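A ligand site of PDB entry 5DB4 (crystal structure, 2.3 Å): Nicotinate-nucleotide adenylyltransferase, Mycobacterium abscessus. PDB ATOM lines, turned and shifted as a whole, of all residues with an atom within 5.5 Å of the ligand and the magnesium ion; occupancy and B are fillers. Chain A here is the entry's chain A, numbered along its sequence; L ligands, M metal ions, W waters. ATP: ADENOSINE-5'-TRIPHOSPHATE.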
ATOM      1  N   MET A  16     -25.414 -15.821 -11.871  1.00  0.00           N
ATOM      2  CA  MET A  16     -24.234 -15.544 -11.032  1.00  0.00           C
ATOM      3  C   MET A  16     -24.378 -14.254 -10.243  1.00  0.00           C
ATOM      4  O   MET A  16     -24.346 -13.139 -10.803  1.00  0.00           O
ATOM      5  CB  MET A  16     -22.961 -15.499 -11.855  1.00  0.00           C
ATOM      6  CG  MET A  16     -21.720 -15.471 -10.976  1.00  0.00           C
ATOM      7  SD  MET A  16     -20.273 -15.584 -12.004  1.00  0.00           S
ATOM      8  CE  MET A  16     -19.045 -16.225 -10.864  1.00  0.00           C
ATOM      9  N   GLY A  17     -24.521 -14.438  -8.927  1.00  0.00           N
ATOM     10  CA  GLY A  17     -24.585 -13.360  -7.966  1.00  0.00           C
ATOM     11  C   GLY A  17     -23.193 -12.878  -7.665  1.00  0.00           C
ATOM     12  O   GLY A  17     -22.216 -13.609  -7.840  1.00  0.00           O
ATOM     13  N   GLY A  18     -23.094 -11.658  -7.193  1.00  0.00           N
ATOM     14  CA  GLY A  18     -21.795 -11.078  -6.875  1.00  0.00           C
ATOM     15  C   GLY A  18     -21.957  -9.637  -6.495  1.00  0.00           C
ATOM     16  O   GLY A  18     -22.955  -8.981  -6.844  1.00  0.00           O
ATOM     17  N   THR A  19     -20.982  -9.136  -5.737  1.00  0.00           N
ATOM     18  CA  THR A  19     -20.949  -7.737  -5.356  1.00  0.00           C
ATOM     19  C   THR A  19     -20.538  -6.927  -6.599  1.00  0.00           C
ATOM     20  O   THR A  19     -21.078  -5.840  -6.834  1.00  0.00           O
ATOM     21  CB  THR A  19     -20.031  -7.507  -4.116  1.00  0.00           C
ATOM     22  OG1 THR A  19     -20.648  -8.083  -2.974  1.00  0.00           O
ATOM     23  CG2 THR A  19     -19.812  -6.033  -3.829  1.00  0.00           C
ATOM     24  N   PHE A  20     -19.627  -7.495  -7.405  1.00  0.00           N
ATOM     25  CA  PHE A  20     -19.214  -6.902  -8.663  1.00  0.00           C
ATOM     26  C   PHE A  20     -18.713  -5.463  -8.466  1.00  0.00           C
ATOM     27  O   PHE A  20     -19.250  -4.496  -9.068  1.00  0.00           O
ATOM     28  CB  PHE A  20     -20.330  -7.015  -9.720  1.00  0.00           C
ATOM     29  CG  PHE A  20     -20.759  -8.440 -10.027  1.00  0.00           C
ATOM     30  CD1 PHE A  20     -19.823  -9.472 -10.254  1.00  0.00           C
ATOM     31  CD2 PHE A  20     -22.088  -8.770 -10.096  1.00  0.00           C
ATOM     32  CE1 PHE A  20     -20.226 -10.768 -10.528  1.00  0.00           C
ATOM     33  CE2 PHE A  20     -22.500 -10.077 -10.389  1.00  0.00           C
ATOM     34  CZ  PHE A  20     -21.571 -11.073 -10.593  1.00  0.00           C
ATOM     35  N   ASP A  21     -17.676  -5.356  -7.625  1.00  0.00           N
ATOM     36  CA  ASP A  21     -17.124  -4.078  -7.188  1.00  0.00           C
ATOM     37  C   ASP A  21     -15.584  -4.086  -7.201  1.00  0.00           C
ATOM     38  O   ASP A  21     -14.965  -3.928  -6.164  1.00  0.00           O
ATOM     39  CB  ASP A  21     -17.642  -3.788  -5.782  1.00  0.00           C
ATOM     40  CG  ASP A  21     -17.410  -2.351  -5.338  1.00  0.00           C
ATOM     41  OD1 ASP A  21     -17.045  -1.485  -6.173  1.00  0.00           O
ATOM     42  OD2 ASP A  21     -17.616  -2.074  -4.131  1.00  0.00           O
ATOM     43  N   HIS A  24     -14.810  -8.726 -12.782  1.00  0.00           N
ATOM     44  CA  HIS A  24     -13.467  -8.979 -13.280  1.00  0.00           C
ATOM     45  C   HIS A  24     -13.452 -10.253 -14.139  1.00  0.00           C
ATOM     46  O   HIS A  24     -14.486 -10.931 -14.309  1.00  0.00           O
ATOM     47  CB  HIS A  24     -12.443  -8.993 -12.132  1.00  0.00           C
ATOM     48  CG  HIS A  24     -12.698 -10.015 -11.059  1.00  0.00           C
ATOM     49  ND1 HIS A  24     -12.553 -11.366 -11.260  1.00  0.00           N
ATOM     50  CD2 HIS A  24     -12.978  -9.866  -9.730  1.00  0.00           C
ATOM     51  CE1 HIS A  24     -12.789 -12.015 -10.126  1.00  0.00           C
ATOM     52  NE2 HIS A  24     -13.040 -11.128  -9.185  1.00  0.00           N
ATOM     53  N   GLY A  26     -11.974 -13.125 -13.809  1.00  0.00           N
ATOM     54  CA  GLY A  26     -12.305 -14.302 -12.994  1.00  0.00           C
ATOM     55  C   GLY A  26     -13.779 -14.636 -12.928  1.00  0.00           C
ATOM     56  O   GLY A  26     -14.157 -15.797 -13.115  1.00  0.00           O
ATOM     57  N   HIS A  27     -14.619 -13.636 -12.654  1.00  0.00           N
ATOM     58  CA  HIS A  27     -16.060 -13.840 -12.635  1.00  0.00           C
ATOM     59  C   HIS A  27     -16.534 -14.270 -14.033  1.00  0.00           C
ATOM     60  O   HIS A  27     -17.283 -15.237 -14.161  1.00  0.00           O
ATOM     61  CB  HIS A  27     -16.805 -12.555 -12.250  1.00  0.00           C
ATOM     62  CG  HIS A  27     -16.491 -12.028 -10.886  1.00  0.00           C
ATOM     63  ND1 HIS A  27     -16.603 -10.699 -10.572  1.00  0.00           N
ATOM     64  CD2 HIS A  27     -16.077 -12.649  -9.757  1.00  0.00           C
ATOM     65  CE1 HIS A  27     -16.283 -10.512  -9.300  1.00  0.00           C
ATOM     66  NE2 HIS A  27     -15.953 -11.678  -8.790  1.00  0.00           N
ATOM     67  N   ALA A  30     -15.422 -17.710 -15.475  1.00  0.00           N
ATOM     68  CA  ALA A  30     -16.093 -18.784 -14.739  1.00  0.00           C
ATOM     69  C   ALA A  30     -17.468 -19.020 -15.321  1.00  0.00           C
ATOM     70  O   ALA A  30     -17.860 -20.171 -15.597  1.00  0.00           O
ATOM     71  CB  ALA A  30     -16.197 -18.410 -13.256  1.00  0.00           C
ATOM     72  N   ARG A  57     -14.930  -1.498   5.010  1.00  0.00           N
ATOM     73  CA  ARG A  57     -15.278  -1.867   3.638  1.00  0.00           C
ATOM     74  C   ARG A  57     -16.398  -0.973   3.078  1.00  0.00           C
ATOM     75  O   ARG A  57     -17.569  -1.144   3.417  1.00  0.00           O
ATOM     76  CB  ARG A  57     -15.692  -3.343   3.581  1.00  0.00           C
ATOM     77  CG  ARG A  57     -16.213  -3.865   2.231  1.00  0.00           C
ATOM     78  CD  ARG A  57     -15.149  -3.914   1.142  1.00  0.00           C
ATOM     79  NE  ARG A  57     -15.609  -4.750   0.016  1.00  0.00           N
ATOM     80  CZ  ARG A  57     -16.141  -4.324  -1.136  1.00  0.00           C
ATOM     81  NH1 ARG A  57     -16.303  -3.024  -1.421  1.00  0.00           N
ATOM     82  NH2 ARG A  57     -16.526  -5.225  -2.035  1.00  0.00           N
ATOM     83  N   ILE A 113     -24.451 -20.248 -10.222  1.00  0.00           N
ATOM     84  CA  ILE A 113     -22.995 -20.374 -10.373  1.00  0.00           C
ATOM     85  C   ILE A 113     -22.301 -19.691  -9.193  1.00  0.00           C
ATOM     86  O   ILE A 113     -22.637 -18.556  -8.818  1.00  0.00           O
ATOM     87  CB  ILE A 113     -22.524 -19.742 -11.707  1.00  0.00           C
ATOM     88  CG1 ILE A 113     -23.316 -20.343 -12.882  1.00  0.00           C
ATOM     89  CG2 ILE A 113     -21.010 -19.885 -11.866  1.00  0.00           C
ATOM     90  CD1 ILE A 113     -22.981 -19.740 -14.234  1.00  0.00           C
ATOM     91  N   THR A 114     -21.335 -20.375  -8.590  1.00  0.00           N
ATOM     92  CA  THR A 114     -20.755 -19.911  -7.320  1.00  0.00           C
ATOM     93  C   THR A 114     -19.362 -20.459  -7.136  1.00  0.00           C
ATOM     94  O   THR A 114     -19.146 -21.637  -7.337  1.00  0.00           O
ATOM     95  CB  THR A 114     -21.662 -20.263  -6.125  1.00  0.00           C
ATOM     96  OG1 THR A 114     -21.293 -19.482  -4.978  1.00  0.00           O
ATOM     97  CG2 THR A 114     -21.613 -21.757  -5.773  1.00  0.00           C
ATOM     98  N   GLY A 115     -18.410 -19.580  -6.793  1.00  0.00           N
ATOM     99  CA  GLY A 115     -17.008 -19.987  -6.569  1.00  0.00           C
ATOM    100  C   GLY A 115     -16.833 -20.631  -5.201  1.00  0.00           C
ATOM    101  O   GLY A 115     -17.740 -20.612  -4.351  1.00  0.00           O
ATOM    102  N   ALA A 116     -15.643 -21.215  -4.983  1.00  0.00           N
ATOM    103  CA  ALA A 116     -15.442 -22.136  -3.857  1.00  0.00           C
ATOM    104  C   ALA A 116     -15.701 -21.477  -2.503  1.00  0.00           C
ATOM    105  O   ALA A 116     -16.328 -22.086  -1.617  1.00  0.00           O
ATOM    106  CB  ALA A 116     -14.057 -22.737  -3.921  1.00  0.00           C
ATOM    107  N   ASP A 117     -15.251 -20.230  -2.339  1.00  0.00           N
ATOM    108  CA  ASP A 117     -15.456 -19.501  -1.090  1.00  0.00           C
ATOM    109  C   ASP A 117     -16.919 -19.261  -0.775  1.00  0.00           C
ATOM    110  O   ASP A 117     -17.358 -19.446   0.359  1.00  0.00           O
ATOM    111  CB  ASP A 117     -14.652 -18.188  -1.043  1.00  0.00           C
ATOM    112  CG  ASP A 117     -15.038 -17.203  -2.141  1.00  0.00           C
ATOM    113  OD1 ASP A 117     -14.843 -17.528  -3.311  1.00  0.00           O
ATOM    114  OD2 ASP A 117     -15.489 -16.081  -1.828  1.00  0.00           O
ATOM    115  N   ALA A 118     -17.693 -18.834  -1.770  1.00  0.00           N
ATOM    116  CA  ALA A 118     -19.108 -18.498  -1.547  1.00  0.00           C
ATOM    117  C   ALA A 118     -19.973 -19.762  -1.398  1.00  0.00           C
ATOM    118  O   ALA A 118     -20.980 -19.735  -0.692  1.00  0.00           O
ATOM    119  CB  ALA A 118     -19.625 -17.602  -2.664  1.00  0.00           C
ATOM    120  N   VAL A 140     -17.730 -23.600  -8.758  1.00  0.00           N
ATOM    121  CA  VAL A 140     -16.557 -23.474  -9.637  1.00  0.00           C
ATOM    122  C   VAL A 140     -15.301 -23.226  -8.815  1.00  0.00           C
ATOM    123  O   VAL A 140     -15.368 -22.712  -7.696  1.00  0.00           O
ATOM    124  CB  VAL A 140     -16.690 -22.353 -10.718  1.00  0.00           C
ATOM    125  CG1 VAL A 140     -17.891 -22.618 -11.640  1.00  0.00           C
ATOM    126  CG2 VAL A 140     -16.789 -20.957 -10.101  1.00  0.00           C
ATOM    127  N   SER A 141     -14.154 -23.567  -9.395  1.00  0.00           N
ATOM    128  CA  SER A 141     -12.884 -23.394  -8.716  1.00  0.00           C
ATOM    129  C   SER A 141     -12.488 -21.906  -8.682  1.00  0.00           C
ATOM    130  O   SER A 141     -12.873 -21.131  -9.554  1.00  0.00           O
ATOM    131  CB  SER A 141     -11.781 -24.237  -9.360  1.00  0.00           C
ATOM    132  OG  SER A 141     -11.640 -23.942 -10.735  1.00  0.00           O
ATOM    133  N   ARG A 142     -11.756 -21.547  -7.628  1.00  0.00           N
ATOM    134  CA  ARG A 142     -11.121 -20.252  -7.491  1.00  0.00           C
ATOM    135  C   ARG A 142      -9.746 -20.481  -6.858  1.00  0.00           C
ATOM    136  O   ARG A 142      -9.676 -21.199  -5.850  1.00  0.00           O
ATOM    137  CB  ARG A 142     -11.960 -19.371  -6.594  1.00  0.00           C
ATOM    138  CG  ARG A 142     -11.444 -17.953  -6.475  1.00  0.00           C
ATOM    139  CD  ARG A 142     -12.389 -17.131  -5.613  1.00  0.00           C
ATOM    140  NE  ARG A 142     -11.971 -15.739  -5.564  1.00  0.00           N
ATOM    141  CZ  ARG A 142     -12.631 -14.762  -4.950  1.00  0.00           C
ATOM    142  NH1 ARG A 142     -13.791 -15.002  -4.315  1.00  0.00           N
ATOM    143  NH2 ARG A 142     -12.135 -13.525  -4.981  1.00  0.00           N
ATOM    144  N   PRO A 143      -8.663 -19.894  -7.442  1.00  0.00           N
ATOM    145  CA  PRO A 143      -7.325 -20.032  -6.851  1.00  0.00           C
ATOM    146  C   PRO A 143      -7.267 -19.573  -5.404  1.00  0.00           C
ATOM    147  O   PRO A 143      -7.859 -18.545  -5.076  1.00  0.00           O
ATOM    148  CB  PRO A 143      -6.444 -19.143  -7.733  1.00  0.00           C
ATOM    149  CG  PRO A 143      -7.123 -19.170  -9.050  1.00  0.00           C
ATOM    150  CD  PRO A 143      -8.595 -19.162  -8.726  1.00  0.00           C
ATOM    151  N   VAL A 167     -12.741 -24.263 -13.643  1.00  0.00           N
ATOM    152  CA  VAL A 167     -12.704 -23.175 -14.634  1.00  0.00           C
ATOM    153  C   VAL A 167     -11.268 -22.657 -14.664  1.00  0.00           C
ATOM    154  O   VAL A 167     -10.509 -22.963 -13.758  1.00  0.00           O
ATOM    155  CB  VAL A 167     -13.752 -22.060 -14.344  1.00  0.00           C
ATOM    156  CG1 VAL A 167     -15.120 -22.707 -14.084  1.00  0.00           C
ATOM    157  CG2 VAL A 167     -13.351 -21.176 -13.179  1.00  0.00           C
ATOM    158  N   LEU A 170      -7.594 -18.017 -12.643  1.00  0.00           N
ATOM    159  CA  LEU A 170      -7.243 -16.585 -12.774  1.00  0.00           C
ATOM    160  C   LEU A 170      -7.298 -16.005 -11.382  1.00  0.00           C
ATOM    161  O   LEU A 170      -8.398 -15.794 -10.821  1.00  0.00           O
ATOM    162  CB  LEU A 170      -8.197 -15.847 -13.718  1.00  0.00           C
ATOM    163  CG  LEU A 170      -8.241 -16.255 -15.216  1.00  0.00           C
ATOM    164  CD1 LEU A 170      -8.908 -15.147 -16.012  1.00  0.00           C
ATOM    165  CD2 LEU A 170      -6.890 -16.603 -15.827  1.00  0.00           C
ATOM    166  N   ALA A 171      -6.107 -15.788 -10.811  1.00  0.00           N
ATOM    167  CA  ALA A 171      -5.993 -15.381  -9.419  1.00  0.00           C
ATOM    168  C   ALA A 171      -6.261 -13.896  -9.345  1.00  0.00           C
ATOM    169  O   ALA A 171      -5.337 -13.086  -9.361  1.00  0.00           O
ATOM    170  CB  ALA A 171      -4.613 -15.732  -8.864  1.00  0.00           C
ATOM    171  N   ILE A 172      -7.552 -13.567  -9.287  1.00  0.00           N
ATOM    172  CA  ILE A 172      -8.063 -12.201  -9.358  1.00  0.00           C
ATOM    173  C   ILE A 172      -9.180 -12.045  -8.346  1.00  0.00           C
ATOM    174  O   ILE A 172     -10.087 -12.880  -8.274  1.00  0.00           O
ATOM    175  CB  ILE A 172      -8.689 -11.875 -10.733  1.00  0.00           C
ATOM    176  CG1 ILE A 172      -7.697 -12.175 -11.867  1.00  0.00           C
ATOM    177  CG2 ILE A 172      -9.163 -10.421 -10.759  1.00  0.00           C
ATOM    178  CD1 ILE A 172      -8.201 -11.835 -13.261  1.00  0.00           C
ATOM    179  N   SER A 173      -9.133 -10.945  -7.589  1.00  0.00           N
ATOM    180  CA  SER A 173     -10.186 -10.575  -6.656  1.00  0.00           C
ATOM    181  C   SER A 173     -10.489  -9.128  -6.875  1.00  0.00           C
ATOM    182  O   SER A 173      -9.633  -8.388  -7.332  1.00  0.00           O
ATOM    183  CB  SER A 173      -9.702 -10.744  -5.204  1.00  0.00           C
ATOM    184  OG  SER A 173      -8.620  -9.849  -4.929  1.00  0.00           O
ATOM    185  N   SER A 174     -11.709  -8.719  -6.535  1.00  0.00           N
ATOM    186  CA  SER A 174     -12.106  -7.335  -6.647  1.00  0.00           C
ATOM    187  C   SER A 174     -11.274  -6.488  -5.672  1.00  0.00           C
ATOM    188  O   SER A 174     -10.854  -5.359  -6.007  1.00  0.00           O
ATOM    189  CB  SER A 174     -13.583  -7.176  -6.342  1.00  0.00           C
ATOM    190  OG  SER A 174     -14.374  -7.947  -7.222  1.00  0.00           O
ATOM    191  N   THR A 175     -11.056  -7.059  -4.492  1.00  0.00           N
ATOM    192  CA  THR A 175     -10.183  -6.497  -3.453  1.00  0.00           C
ATOM    193  C   THR A 175      -8.859  -6.042  -4.013  1.00  0.00           C
ATOM    194  O   THR A 175      -8.488  -4.888  -3.859  1.00  0.00           O
ATOM    195  CB  THR A 175      -9.967  -7.490  -2.285  1.00  0.00           C
ATOM    196  OG1 THR A 175     -11.229  -7.700  -1.616  1.00  0.00           O
ATOM    197  CG2 THR A 175      -8.931  -6.953  -1.252  1.00  0.00           C
ATOM    198  N   ASP A 176      -8.155  -6.954  -4.669  1.00  0.00           N
ATOM    199  CA  ASP A 176      -6.897  -6.618  -5.303  1.00  0.00           C
ATOM    200  C   ASP A 176      -7.106  -5.481  -6.305  1.00  0.00           C
ATOM    201  O   ASP A 176      -6.372  -4.515  -6.276  1.00  0.00           O
ATOM    202  CB  ASP A 176      -6.275  -7.825  -5.980  1.00  0.00           C
ATOM    203  CG  ASP A 176      -4.883  -7.545  -6.494  1.00  0.00           C
ATOM    204  OD1 ASP A 176      -4.019  -7.135  -5.692  1.00  0.00           O
ATOM    205  OD2 ASP A 176      -4.634  -7.714  -7.715  1.00  0.00           O
ATOM    206  N   ARG A 178      -9.538  -3.092  -6.356  1.00  0.00           N
ATOM    207  CA  ARG A 178      -9.781  -1.879  -5.548  1.00  0.00           C
ATOM    208  C   ARG A 178      -8.499  -1.269  -4.941  1.00  0.00           C
ATOM    209  O   ARG A 178      -8.328  -0.049  -4.933  1.00  0.00           O
ATOM    210  CB  ARG A 178     -10.784  -2.155  -4.432  1.00  0.00           C
ATOM    211  CG  ARG A 178     -12.219  -2.338  -4.890  1.00  0.00           C
ATOM    212  CD  ARG A 178     -13.159  -2.355  -3.700  1.00  0.00           C
ATOM    213  NE  ARG A 178     -12.836  -3.451  -2.763  1.00  0.00           N
ATOM    214  CZ  ARG A 178     -13.254  -4.720  -2.845  1.00  0.00           C
ATOM    215  NH1 ARG A 178     -14.055  -5.143  -3.840  1.00  0.00           N
ATOM    216  NH2 ARG A 178     -12.874  -5.603  -1.936  1.00  0.00           N
HETATM  217  PG  ATP L   1     -14.016  -9.342  -3.038  1.00  0.00           P
HETATM  218  O1G ATP L   1     -14.653 -10.288  -2.060  1.00  0.00           O
HETATM  219  O2G ATP L   1     -14.361  -7.907  -2.732  1.00  0.00           O
HETATM  220  O3G ATP L   1     -12.528  -9.619  -3.158  1.00  0.00           O
HETATM  221  PB  ATP L   1     -14.529 -11.011  -5.304  1.00  0.00           P
HETATM  222  O1B ATP L   1     -14.350 -12.078  -4.214  1.00  0.00           O
HETATM  223  O2B ATP L   1     -13.512 -11.152  -6.375  1.00  0.00           O
HETATM  224  O3B ATP L   1     -14.485  -9.617  -4.549  1.00  0.00           O
HETATM  225  PA  ATP L   1     -17.384 -11.376  -5.257  1.00  0.00           P
HETATM  226  O1A ATP L   1     -17.170 -11.429  -3.735  1.00  0.00           O
HETATM  227  O2A ATP L   1     -18.370 -10.351  -5.651  1.00  0.00           O
HETATM  228  O3A ATP L   1     -15.992 -11.021  -5.914  1.00  0.00           O
HETATM  229  O5' ATP L   1     -17.623 -12.826  -5.818  1.00  0.00           O
HETATM  230  C5' ATP L   1     -18.901 -13.191  -6.356  1.00  0.00           C
HETATM  231  C4' ATP L   1     -18.794 -14.593  -6.877  1.00  0.00           C
HETATM  232  O4' ATP L   1     -17.615 -14.694  -7.721  1.00  0.00           O
HETATM  233  C3' ATP L   1     -18.644 -15.672  -5.796  1.00  0.00           C
HETATM  234  O3' ATP L   1     -19.410 -16.827  -6.128  1.00  0.00           O
HETATM  235  C2' ATP L   1     -17.143 -15.949  -5.816  1.00  0.00           C
HETATM  236  O2' ATP L   1     -16.826 -17.229  -5.304  1.00  0.00           O
HETATM  237  C1' ATP L   1     -16.848 -15.807  -7.302  1.00  0.00           C
HETATM  238  N9  ATP L   1     -15.456 -15.525  -7.628  1.00  0.00           N
HETATM  239  C8  ATP L   1     -14.754 -14.403  -7.288  1.00  0.00           C
HETATM  240  N7  ATP L   1     -13.562 -14.328  -7.828  1.00  0.00           N
HETATM  241  C5  ATP L   1     -13.466 -15.489  -8.567  1.00  0.00           C
HETATM  242  C6  ATP L   1     -12.459 -15.994  -9.419  1.00  0.00           C
HETATM  243  N6  ATP L   1     -11.276 -15.407  -9.589  1.00  0.00           N
HETATM  244  N1  ATP L   1     -12.703 -17.159 -10.051  1.00  0.00           N
HETATM  245  C2  ATP L   1     -13.855 -17.800  -9.816  1.00  0.00           C
HETATM  246  N3  ATP L   1     -14.877 -17.420  -9.030  1.00  0.00           N
HETATM  247  C4  ATP L   1     -14.619 -16.246  -8.445  1.00  0.00           C
HETATM  248 MG    MG M   1     -15.504 -12.091  -2.481  1.00  0.00          MG
HETATM  249  O   HOH W   1     -14.851  -9.960   0.935  1.00  0.00           O
HETATM  250  O   HOH W   2      -9.223 -15.812  -6.913  1.00  0.00           O
HETATM  251  O   HOH W   3     -10.491 -18.661 -11.549  1.00  0.00           O
HETATM  252  O   HOH W   4     -16.588  -7.418  -3.564  1.00  0.00           O
HETATM  253  O   HOH W   5     -16.600 -13.897  -2.993  1.00  0.00           O
HETATM  254  O   HOH W   6     -16.892 -12.102  -0.903  1.00  0.00           O
HETATM  255  O   HOH W   7     -11.597 -11.599  -1.985  1.00  0.00           O
HETATM  256  O   HOH W   8     -16.670  -7.912  -6.388  1.00  0.00           O
HETATM  257  O   HOH W   9     -13.918 -13.189  -1.727  1.00  0.00           O
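An oxygen (O2G) of the ligand lies within salt-bridge range of the guanidinium group (NH2) of Arg 178, at 2.9 Å.
A nitrogen (N6) of the ligand is in hydrogen-bond range of the backbone carbonyl oxygen (O) of Ile 172, at 3.1 Å.
N of Gly 115 lies within hydrogen-bond range of O3' of the ligand (3.0 Å).
O2B of the ligand sits at hydrogen-bond distance from NE2 of His 24 (2.8 Å).
The side-chain carboxylate of Asp 117 is in hydrogen-bond range of an oxygen (O2') of the ligand.
The backbone carbonyl oxygen of Leu 170 sits at hydrogen-bond distance from a nitrogen (N6) of the ligand (3.2 Å).
The side-chain hydroxyl (OG1) of Thr 114 lies within hydrogen-bond range of an oxygen (O3') of the ligand.
An oxygen (O3G) of the ligand lies within hydrogen-bond range of the side-chain hydroxyl (OG1) of Thr 175 (2.8 Å).
A ring nitrogen (NE2) of His 27 sits at hydrogen-bond distance from an oxygen (O3A) of the ligand, 3.0 Å away.
The side-chain hydroxyl (OG) of Ser 174 sits at hydrogen-bond distance from an oxygen (O3B) of the ligand (3.2 Å).
The backbone NH of Thr 19 is in hydrogen-bond range of an oxygen (O2A) of the ligand (2.9 Å).
O3G of the ligand sits at hydrogen-bond distance from N of Thr 175 (3.2 Å).
NH2 of Arg 142 lies within salt-bridge range of O2B of the ligand, at 3.1 Å.
The backbone NH (N) of Ser 174 lies within hydrogen-bond range of an oxygen (O2B) of the ligand.
NH2 of Arg 57 is in salt-bridge range of O2G of the ligand (3.5 Å).
OG of Ser 173 is in hydrogen-bond range of N of Asp 176, at 2.9 Å.
The guanidinium group (NH1) of Arg 178 sits at hydrogen-bond distance from the backbone carbonyl oxygen (O) of Asp 21 (2.8 Å).
ND1 of His 24 is in hydrogen-bond range of N of Gly 26, 3.2 Å away.
The side-chain hydroxyl (OG) of Ser 141 sits at hydrogen-bond distance from the backbone NH (N) of Val 167 (3.1 Å).
The side-chain hydroxyl (OG1) of Thr 175 sits at hydrogen-bond distance from the guanidinium group (NH2) of Arg 178.
N of Val 140 is in hydrogen-bond range of O of Thr 114.
The guanidinium group (NH1) of Arg 57 is in salt-bridge range of the side-chain carboxylate (OD2) of Asp 21, at 3.2 Å.
The guanidinium group (NH1) of Arg 142 is in salt-bridge range of the side-chain carboxylate (OD1) of Asp 117, at 2.9 Å.
CE of Met 16 touches O4' of the ligand, 3.8 Å away.
O of Gly 17 touches C5' of the ligand (3.7 Å).
Gly 18 touches the ligand (CA to C5', 3.6 Å).
N of Phe 20 touches O2A of the ligand, 3.6 Å away.
O of Gly 26 touches N1 of the ligand, 3.7 Å away.
Ala 118 touches the ligand.
Ser 141 touches the ligand.
Ser 173 touches the ligand (CA to O2B, 3.4 Å).
Hydrophobic or aromatic side chains that line the ligand: Met 16, His 24, His 27 and Ala 118.
21 residues have an atom within 4 Å of the ligand: Met 16, Gly 17, Gly 18, Thr 19, Phe 20, His 24, Gly 26, His 27, Arg 57, Thr 114, Gly 115, Asp 117, Ala 118, Ser 141, Arg 142, Leu 170, Ile 172, Ser 173, Ser 174, Thr 175 and Arg 178.
The nearest printed residue that does not touch the ligand is Val 140 (4.2 Å).
Arg 142 touches the magnesium ion.
Of the 30 residues printed, 1 comes within 4 Å of the magnesium ion.
O1G of the ligand binds the magnesium ion (2.0 Å).
Water W9 binds the magnesium ion.
O1B of the ligand is bound to the magnesium ion, at 2.1 Å.
The magnesium ion is bound by water W6 (2.1 Å).
Water W5 binds the magnesium ion (2.2 Å).
O1A of the ligand binds the magnesium ion.
Water W9 lies within hydrogen-bond range of the guanidinium group of Arg 142 (3.2 Å) and the side-chain carboxylate of Asp 117 (3.3 Å).
Water W5 lies within hydrogen-bond range of the side-chain carboxylate (OD2) of Asp 117 (2.7 Å), an oxygen (O5') of the ligand (3.2 Å) and the guanidinium group (NH1) of Arg 142 (3.3 Å).
Water W4 lies within hydrogen-bond range of O2G of the ligand (2.4 Å), NH2 of Arg 57 (2.7 Å) and NH1 of Arg 178 (3.4 Å).
Water W8 lies within hydrogen-bond range of the side-chain hydroxyl (OG) of Ser 174 (2.4 Å), the backbone NH (N) of Asp 21 (3.0 Å), an oxygen (O2A) of the ligand (3.1 Å) and the backbone NH (N) of Phe 20 (3.2 Å).
Water W3 lies within hydrogen-bond range of a nitrogen (N1) of the ligand (3.1 Å) and the backbone NH of Leu 170 (3.2 Å).
Water W2 lies within hydrogen-bond range of the guanidinium group (NE) of Arg 142 (3.1 Å), the backbone carbonyl oxygen (O) of Ile 172 (3.3 Å) and a nitrogen (N6) of the ligand (3.4 Å).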
